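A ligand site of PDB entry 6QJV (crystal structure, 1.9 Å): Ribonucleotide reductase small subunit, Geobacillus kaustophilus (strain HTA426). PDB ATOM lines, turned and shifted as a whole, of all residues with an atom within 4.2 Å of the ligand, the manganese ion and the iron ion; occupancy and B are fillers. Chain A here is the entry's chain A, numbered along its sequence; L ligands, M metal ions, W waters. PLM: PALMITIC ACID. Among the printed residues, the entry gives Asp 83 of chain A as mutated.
The side-chain hydroxyl of Thr 191 lies within hydrogen-bond range of the backbone carbonyl oxygen of Ser 187.
N of Ala 185 lies within hydrogen-bond range of O of Val 180, 2.8 Å away.
Merely in contact with the ligand: Gly 78 (3.4 Å), Phe 149 (3.5 Å), Thr 191 (3.5 Å), Leu 184 (3.6 Å), Phe 79 (3.6 Å), Val 86 (3.6 Å), Val 180 (3.7 Å), Leu 75 (3.7 Å), Gly 188 (3.8 Å) and Tyr 255 (3.9 Å).
Hydrophobic or aromatic side chains that line the ligand: Leu 75, Phe 79, Val 86, Phe 149, Val 180 and Tyr 255.
Along chain A the residues within 4 Å of the ligand span positions 75 to 255.
Of the 23 residues printed, 3 come within 4 Å of the manganese ion.
Along chain A the residues within 4 Å of the manganese ion span positions 83 to 119.
Four residues have an atom within 4 Å of the iron ion: Glu 116, Glu 181, Glu 216 and His 219.
Along chain A the residues within 4 Å of the iron ion span positions 116 to 219.
The nearest printed residue that does not touch the iron ion is Phe 112 (4.1 Å).
O2 of the ligand binds the manganese ion (1.8 Å).
OD1 of Asp 83 binds the manganese ion (2.1 Å).
The manganese ion is bound by water W2 (2.1 Å).
The side-chain carboxylate (OE2) of Glu 116 binds the manganese ion (2.1 Å).
ND1 of His 119 binds the manganese ion, at 2.2 Å.
The manganese ion is bound by water W1, 2.3 Å away.
The manganese ion has six donor atoms within binding distance.
The iron ion is bound by water W2 (2.0 Å), OE2 of Glu 181 (2.0 Å), O1 of the ligand (2.1 Å), OE1 of Glu 116 (2.1 Å), OE2 of Glu 216 (2.2 Å) and ND1 of His 219 (2.2 Å).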
ATOM      1  N   LEU A  75     -17.711  15.043 -17.755  1.00  0.00           N
ATOM      2  CA  LEU A  75     -16.724  15.206 -18.812  1.00  0.00           C
ATOM      3  C   LEU A  75     -16.142  16.615 -18.793  1.00  0.00           C
ATOM      4  O   LEU A  75     -14.940  16.793 -19.004  1.00  0.00           O
ATOM      5  CB  LEU A  75     -17.369  14.914 -20.164  1.00  0.00           C
ATOM      6  CG  LEU A  75     -16.496  14.602 -21.375  1.00  0.00           C
ATOM      7  CD1 LEU A  75     -15.703  13.301 -21.171  1.00  0.00           C
ATOM      8  CD2 LEU A  75     -17.380  14.532 -22.654  1.00  0.00           C
ATOM      9  N   GLY A  78     -13.663  16.778 -16.004  1.00  0.00           N
ATOM     10  CA  GLY A  78     -12.388  16.187 -16.345  1.00  0.00           C
ATOM     11  C   GLY A  78     -11.543  17.103 -17.216  1.00  0.00           C
ATOM     12  O   GLY A  78     -10.332  17.217 -17.018  1.00  0.00           O
ATOM     13  N   PHE A  79     -12.173  17.781 -18.179  1.00  0.00           N
ATOM     14  CA  PHE A  79     -11.430  18.665 -19.057  1.00  0.00           C
ATOM     15  C   PHE A  79     -10.972  19.931 -18.370  1.00  0.00           C
ATOM     16  O   PHE A  79      -9.849  20.372 -18.592  1.00  0.00           O
ATOM     17  CB  PHE A  79     -12.242  19.006 -20.298  1.00  0.00           C
ATOM     18  CG  PHE A  79     -11.951  18.106 -21.466  1.00  0.00           C
ATOM     19  CD1 PHE A  79     -10.777  18.268 -22.188  1.00  0.00           C
ATOM     20  CD2 PHE A  79     -12.834  17.095 -21.839  1.00  0.00           C
ATOM     21  CE1 PHE A  79     -10.481  17.421 -23.258  1.00  0.00           C
ATOM     22  CE2 PHE A  79     -12.526  16.262 -22.925  1.00  0.00           C
ATOM     23  CZ  PHE A  79     -11.350  16.422 -23.609  1.00  0.00           C
ATOM     24  N   GLY A  82      -8.164  19.157 -16.244  1.00  0.00           N
ATOM     25  CA  GLY A  82      -7.060  18.657 -17.050  1.00  0.00           C
ATOM     26  C   GLY A  82      -6.341  19.779 -17.792  1.00  0.00           C
ATOM     27  O   GLY A  82      -5.102  19.856 -17.800  1.00  0.00           O
ATOM     28  N   ASP A  83      -7.107  20.689 -18.397  1.00  0.00           N
ATOM     29  CA  ASP A  83      -6.498  21.814 -19.086  1.00  0.00           C
ATOM     30  C   ASP A  83      -5.801  22.757 -18.112  1.00  0.00           C
ATOM     31  O   ASP A  83      -4.735  23.311 -18.426  1.00  0.00           O
ATOM     32  CB  ASP A  83      -7.537  22.530 -19.933  1.00  0.00           C
ATOM     33  CG  ASP A  83      -7.592  21.961 -21.348  1.00  0.00           C
ATOM     34  OD1 ASP A  83      -6.540  21.950 -21.992  1.00  0.00           O
ATOM     35  OD2 ASP A  83      -8.641  21.495 -21.806  1.00  0.00           O
ATOM     36  N   VAL A  86      -2.416  20.962 -17.204  1.00  0.00           N
ATOM     37  CA  VAL A  86      -1.372  21.001 -18.240  1.00  0.00           C
ATOM     38  C   VAL A  86      -0.885  22.422 -18.513  1.00  0.00           C
ATOM     39  O   VAL A  86       0.265  22.607 -18.919  1.00  0.00           O
ATOM     40  CB  VAL A  86      -1.831  20.298 -19.541  1.00  0.00           C
ATOM     41  CG1 VAL A  86      -2.106  18.832 -19.282  1.00  0.00           C
ATOM     42  CG2 VAL A  86      -3.027  20.941 -20.163  1.00  0.00           C
ATOM     43  N   PHE A 112       2.432  26.186 -27.367  1.00  0.00           N
ATOM     44  CA  PHE A 112       1.825  25.090 -26.603  1.00  0.00           C
ATOM     45  C   PHE A 112       1.164  25.633 -25.338  1.00  0.00           C
ATOM     46  O   PHE A 112      -0.012  25.360 -25.044  1.00  0.00           O
ATOM     47  CB  PHE A 112       2.935  24.068 -26.281  1.00  0.00           C
ATOM     48  CG  PHE A 112       2.489  22.683 -25.878  1.00  0.00           C
ATOM     49  CD1 PHE A 112       3.259  21.583 -26.236  1.00  0.00           C
ATOM     50  CD2 PHE A 112       1.384  22.453 -25.079  1.00  0.00           C
ATOM     51  CE1 PHE A 112       2.901  20.302 -25.875  1.00  0.00           C
ATOM     52  CE2 PHE A 112       1.035  21.162 -24.690  1.00  0.00           C
ATOM     53  CZ  PHE A 112       1.821  20.088 -25.075  1.00  0.00           C
ATOM     54  N   GLU A 116      -2.950  26.044 -24.211  1.00  0.00           N
ATOM     55  CA  GLU A 116      -3.603  25.449 -23.048  1.00  0.00           C
ATOM     56  C   GLU A 116      -4.292  26.514 -22.214  1.00  0.00           C
ATOM     57  O   GLU A 116      -5.343  26.257 -21.635  1.00  0.00           O
ATOM     58  CB  GLU A 116      -2.595  24.694 -22.196  1.00  0.00           C
ATOM     59  CG  GLU A 116      -1.816  23.527 -22.891  1.00  0.00           C
ATOM     60  CD  GLU A 116      -2.725  22.360 -23.327  1.00  0.00           C
ATOM     61  OE1 GLU A 116      -2.213  21.306 -23.754  1.00  0.00           O
ATOM     62  OE2 GLU A 116      -3.945  22.469 -23.212  1.00  0.00           O
ATOM     63  N   HIS A 119      -7.523  26.922 -23.673  1.00  0.00           N
ATOM     64  CA  HIS A 119      -8.389  25.783 -23.369  1.00  0.00           C
ATOM     65  C   HIS A 119      -9.053  25.946 -22.008  1.00  0.00           C
ATOM     66  O   HIS A 119     -10.259  25.712 -21.857  1.00  0.00           O
ATOM     67  CB  HIS A 119      -7.590  24.485 -23.417  1.00  0.00           C
ATOM     68  CG  HIS A 119      -7.037  24.190 -24.769  1.00  0.00           C
ATOM     69  ND1 HIS A 119      -6.271  23.070 -25.029  1.00  0.00           N
ATOM     70  CD2 HIS A 119      -7.109  24.883 -25.930  1.00  0.00           C
ATOM     71  CE1 HIS A 119      -5.914  23.087 -26.312  1.00  0.00           C
ATOM     72  NE2 HIS A 119      -6.396  24.186 -26.868  1.00  0.00           N
ATOM     73  N   PHE A 149      -3.878  13.198 -12.717  1.00  0.00           N
ATOM     74  CA  PHE A 149      -3.838  14.653 -12.876  1.00  0.00           C
ATOM     75  C   PHE A 149      -3.396  15.409 -11.631  1.00  0.00           C
ATOM     76  O   PHE A 149      -2.763  16.469 -11.751  1.00  0.00           O
ATOM     77  CB  PHE A 149      -5.216  15.154 -13.313  1.00  0.00           C
ATOM     78  CG  PHE A 149      -5.519  14.855 -14.770  1.00  0.00           C
ATOM     79  CD1 PHE A 149      -5.076  15.732 -15.762  1.00  0.00           C
ATOM     80  CD2 PHE A 149      -6.200  13.701 -15.142  1.00  0.00           C
ATOM     81  CE1 PHE A 149      -5.304  15.469 -17.075  1.00  0.00           C
ATOM     82  CE2 PHE A 149      -6.439  13.430 -16.489  1.00  0.00           C
ATOM     83  CZ  PHE A 149      -5.995  14.337 -17.443  1.00  0.00           C
ATOM     84  N   VAL A 180      -2.125  11.785 -21.143  1.00  0.00           N
ATOM     85  CA  VAL A 180      -3.116  12.806 -20.844  1.00  0.00           C
ATOM     86  C   VAL A 180      -3.733  13.363 -22.143  1.00  0.00           C
ATOM     87  O   VAL A 180      -4.961  13.484 -22.266  1.00  0.00           O
ATOM     88  CB  VAL A 180      -2.485  13.919 -19.971  1.00  0.00           C
ATOM     89  CG1 VAL A 180      -3.277  15.197 -20.001  1.00  0.00           C
ATOM     90  CG2 VAL A 180      -2.342  13.416 -18.542  1.00  0.00           C
ATOM     91  N   GLU A 181      -2.905  13.757 -23.102  1.00  0.00           N
ATOM     92  CA  GLU A 181      -3.357  14.319 -24.374  1.00  0.00           C
ATOM     93  C   GLU A 181      -3.678  13.229 -25.396  1.00  0.00           C
ATOM     94  O   GLU A 181      -4.785  13.196 -25.948  1.00  0.00           O
ATOM     95  CB  GLU A 181      -2.312  15.275 -24.941  1.00  0.00           C
ATOM     96  CG  GLU A 181      -1.974  16.471 -24.028  1.00  0.00           C
ATOM     97  CD  GLU A 181      -0.957  17.401 -24.600  1.00  0.00           C
ATOM     98  OE1 GLU A 181       0.100  16.895 -25.020  1.00  0.00           O
ATOM     99  OE2 GLU A 181      -1.231  18.633 -24.644  1.00  0.00           O
ATOM    100  N   LEU A 184      -6.289  10.269 -23.290  1.00  0.00           N
ATOM    101  CA  LEU A 184      -7.508  10.752 -22.631  1.00  0.00           C
ATOM    102  C   LEU A 184      -8.144  11.934 -23.367  1.00  0.00           C
ATOM    103  O   LEU A 184      -9.345  11.925 -23.632  1.00  0.00           O
ATOM    104  CB  LEU A 184      -7.196  11.124 -21.174  1.00  0.00           C
ATOM    105  CG  LEU A 184      -6.936   9.963 -20.224  1.00  0.00           C
ATOM    106  CD1 LEU A 184      -6.473  10.496 -18.857  1.00  0.00           C
ATOM    107  CD2 LEU A 184      -8.145   9.114 -20.042  1.00  0.00           C
ATOM    108  N   ALA A 185      -7.370  12.978 -23.686  1.00  0.00           N
ATOM    109  CA  ALA A 185      -7.977  14.149 -24.330  1.00  0.00           C
ATOM    110  C   ALA A 185      -8.628  13.771 -25.677  1.00  0.00           C
ATOM    111  O   ALA A 185      -9.755  14.197 -25.986  1.00  0.00           O
ATOM    112  CB  ALA A 185      -6.942  15.243 -24.553  1.00  0.00           C
ATOM    113  N   SER A 187      -9.762  10.935 -26.699  1.00  0.00           N
ATOM    114  CA  SER A 187     -10.968  10.158 -26.475  1.00  0.00           C
ATOM    115  C   SER A 187     -12.081  11.041 -25.939  1.00  0.00           C
ATOM    116  O   SER A 187     -13.245  10.842 -26.301  1.00  0.00           O
ATOM    117  CB  SER A 187     -10.687   9.000 -25.512  1.00  0.00           C
ATOM    118  OG  SER A 187      -9.649   8.162 -26.013  1.00  0.00           O
ATOM    119  N   GLY A 188     -11.735  12.056 -25.164  1.00  0.00           N
ATOM    120  CA  GLY A 188     -12.734  13.007 -24.707  1.00  0.00           C
ATOM    121  C   GLY A 188     -13.356  13.818 -25.825  1.00  0.00           C
ATOM    122  O   GLY A 188     -14.577  14.048 -25.827  1.00  0.00           O
ATOM    123  N   THR A 191     -15.670  11.579 -27.606  1.00  0.00           N
ATOM    124  CA  THR A 191     -16.881  11.328 -26.819  1.00  0.00           C
ATOM    125  C   THR A 191     -17.856  12.493 -26.926  1.00  0.00           C
ATOM    126  O   THR A 191     -19.045  12.293 -27.166  1.00  0.00           O
ATOM    127  CB  THR A 191     -16.494  11.050 -25.362  1.00  0.00           C
ATOM    128  OG1 THR A 191     -15.708   9.859 -25.301  1.00  0.00           O
ATOM    129  CG2 THR A 191     -17.690  10.837 -24.465  1.00  0.00           C
ATOM    130  N   GLU A 216      -4.493  20.151 -30.369  1.00  0.00           N
ATOM    131  CA  GLU A 216      -3.972  18.960 -29.711  1.00  0.00           C
ATOM    132  C   GLU A 216      -3.079  18.170 -30.624  1.00  0.00           C
ATOM    133  O   GLU A 216      -2.139  17.526 -30.157  1.00  0.00           O
ATOM    134  CB  GLU A 216      -5.095  18.011 -29.256  1.00  0.00           C
ATOM    135  CG  GLU A 216      -4.699  17.065 -28.152  1.00  0.00           C
ATOM    136  CD  GLU A 216      -4.558  17.866 -26.880  1.00  0.00           C
ATOM    137  OE1 GLU A 216      -5.617  18.220 -26.315  1.00  0.00           O
ATOM    138  OE2 GLU A 216      -3.405  18.175 -26.527  1.00  0.00           O
ATOM    139  N   HIS A 219       0.367  19.340 -30.023  1.00  0.00           N
ATOM    140  CA  HIS A 219       0.850  18.909 -28.716  1.00  0.00           C
ATOM    141  C   HIS A 219       1.330  17.465 -28.756  1.00  0.00           C
ATOM    142  O   HIS A 219       2.408  17.118 -28.232  1.00  0.00           O
ATOM    143  CB  HIS A 219      -0.263  19.100 -27.661  1.00  0.00           C
ATOM    144  CG  HIS A 219      -0.816  20.489 -27.606  1.00  0.00           C
ATOM    145  ND1 HIS A 219      -1.866  20.848 -26.783  1.00  0.00           N
ATOM    146  CD2 HIS A 219      -0.472  21.607 -28.290  1.00  0.00           C
ATOM    147  CE1 HIS A 219      -2.125  22.138 -26.958  1.00  0.00           C
ATOM    148  NE2 HIS A 219      -1.298  22.616 -27.878  1.00  0.00           N
ATOM    149  N   TYR A 255     -10.505   5.395 -14.749  1.00  0.00           N
ATOM    150  CA  TYR A 255     -11.300   6.602 -14.927  1.00  0.00           C
ATOM    151  C   TYR A 255     -12.363   6.383 -15.999  1.00  0.00           C
ATOM    152  O   TYR A 255     -13.512   6.805 -15.836  1.00  0.00           O
ATOM    153  CB  TYR A 255     -10.388   7.772 -15.251  1.00  0.00           C
ATOM    154  CG  TYR A 255     -11.103   9.073 -15.537  1.00  0.00           C
ATOM    155  CD1 TYR A 255     -11.939   9.651 -14.589  1.00  0.00           C
ATOM    156  CD2 TYR A 255     -10.921   9.733 -16.738  1.00  0.00           C
ATOM    157  CE1 TYR A 255     -12.584  10.884 -14.864  1.00  0.00           C
ATOM    158  CE2 TYR A 255     -11.576  10.956 -17.010  1.00  0.00           C
ATOM    159  CZ  TYR A 255     -12.386  11.518 -16.061  1.00  0.00           C
ATOM    160  OH  TYR A 255     -13.008  12.742 -16.357  1.00  0.00           O
ATOM    161  N   VAL A 256     -12.010   5.732 -17.115  1.00  0.00           N
ATOM    162  CA  VAL A 256     -12.974   5.527 -18.186  1.00  0.00           C
ATOM    163  C   VAL A 256     -14.153   4.695 -17.665  1.00  0.00           C
ATOM    164  O   VAL A 256     -15.318   5.045 -17.877  1.00  0.00           O
ATOM    165  CB  VAL A 256     -12.305   4.884 -19.410  1.00  0.00           C
ATOM    166  CG1 VAL A 256     -13.343   4.404 -20.444  1.00  0.00           C
ATOM    167  CG2 VAL A 256     -11.348   5.836 -20.084  1.00  0.00           C
ATOM    168  N   LEU A 259     -16.458   6.921 -15.497  1.00  0.00           N
ATOM    169  CA  LEU A 259     -17.334   7.774 -16.296  1.00  0.00           C
ATOM    170  C   LEU A 259     -18.409   6.949 -16.985  1.00  0.00           C
ATOM    171  O   LEU A 259     -19.536   7.406 -17.189  1.00  0.00           O
ATOM    172  CB  LEU A 259     -16.545   8.516 -17.361  1.00  0.00           C
ATOM    173  CG  LEU A 259     -15.565   9.561 -16.847  1.00  0.00           C
ATOM    174  CD1 LEU A 259     -14.887  10.151 -18.043  1.00  0.00           C
ATOM    175  CD2 LEU A 259     -16.282  10.643 -16.051  1.00  0.00           C
ATOM    176  N   LEU A 282     -17.020   3.513 -26.997  1.00  0.00           N
ATOM    177  CA  LEU A 282     -16.129   4.534 -26.455  1.00  0.00           C
ATOM    178  C   LEU A 282     -14.936   3.883 -25.769  1.00  0.00           C
ATOM    179  O   LEU A 282     -13.792   4.337 -25.908  1.00  0.00           O
ATOM    180  CB  LEU A 282     -16.879   5.442 -25.489  1.00  0.00           C
ATOM    181  CG  LEU A 282     -18.052   6.248 -26.069  1.00  0.00           C
ATOM    182  CD1 LEU A 282     -18.820   6.966 -24.965  1.00  0.00           C
ATOM    183  CD2 LEU A 282     -17.594   7.242 -27.138  1.00  0.00           C
HETATM  184  C1  PLM L   1      -4.774  19.012 -22.687  1.00  0.00           C
HETATM  185  O1  PLM L   1      -3.697  18.878 -23.390  1.00  0.00           O
HETATM  186  O2  PLM L   1      -5.543  19.993 -22.630  1.00  0.00           O
HETATM  187  C2  PLM L   1      -5.150  17.802 -21.758  1.00  0.00           C
HETATM  188  C3  PLM L   1      -6.604  17.680 -21.380  1.00  0.00           C
HETATM  189  C4  PLM L   1      -6.911  16.512 -20.523  1.00  0.00           C
HETATM  190  C5  PLM L   1      -8.379  16.166 -20.509  1.00  0.00           C
HETATM  191  C6  PLM L   1      -8.717  15.116 -19.498  1.00  0.00           C
HETATM  192  C7  PLM L   1     -10.202  14.796 -19.421  1.00  0.00           C
HETATM  193  C8  PLM L   1     -10.644  14.076 -20.611  1.00  0.00           C
HETATM  194  C9  PLM L   1     -11.837  13.192 -20.391  1.00  0.00           C
HETATM  195  CA  PLM L   1     -11.550  11.735 -20.794  1.00  0.00           C
HETATM  196  CB  PLM L   1     -12.741  11.079 -21.377  1.00  0.00           C
HETATM  197  CC  PLM L   1     -12.485   9.658 -21.874  1.00  0.00           C
HETATM  198  CD  PLM L   1     -13.749   9.029 -22.471  1.00  0.00           C
HETATM  199  CE  PLM L   1     -14.532   8.134 -21.530  1.00  0.00           C
HETATM  200  CF  PLM L   1     -15.829   7.546 -22.138  1.00  0.00           C
HETATM  201  CG  PLM L   1     -17.132   7.922 -21.362  1.00  0.00           C
HETATM  202 MN    MN M   1      -5.685  21.371 -23.766  1.00  0.00          MN
HETATM  203 FE    FE M   2      -2.828  19.772 -25.061  1.00  0.00          FE
HETATM  204  O   HOH W   1      -7.712  20.377 -24.079  1.00  0.00           O
HETATM  205  O   HOH W   2      -4.680  20.344 -25.281  1.00  0.00           O
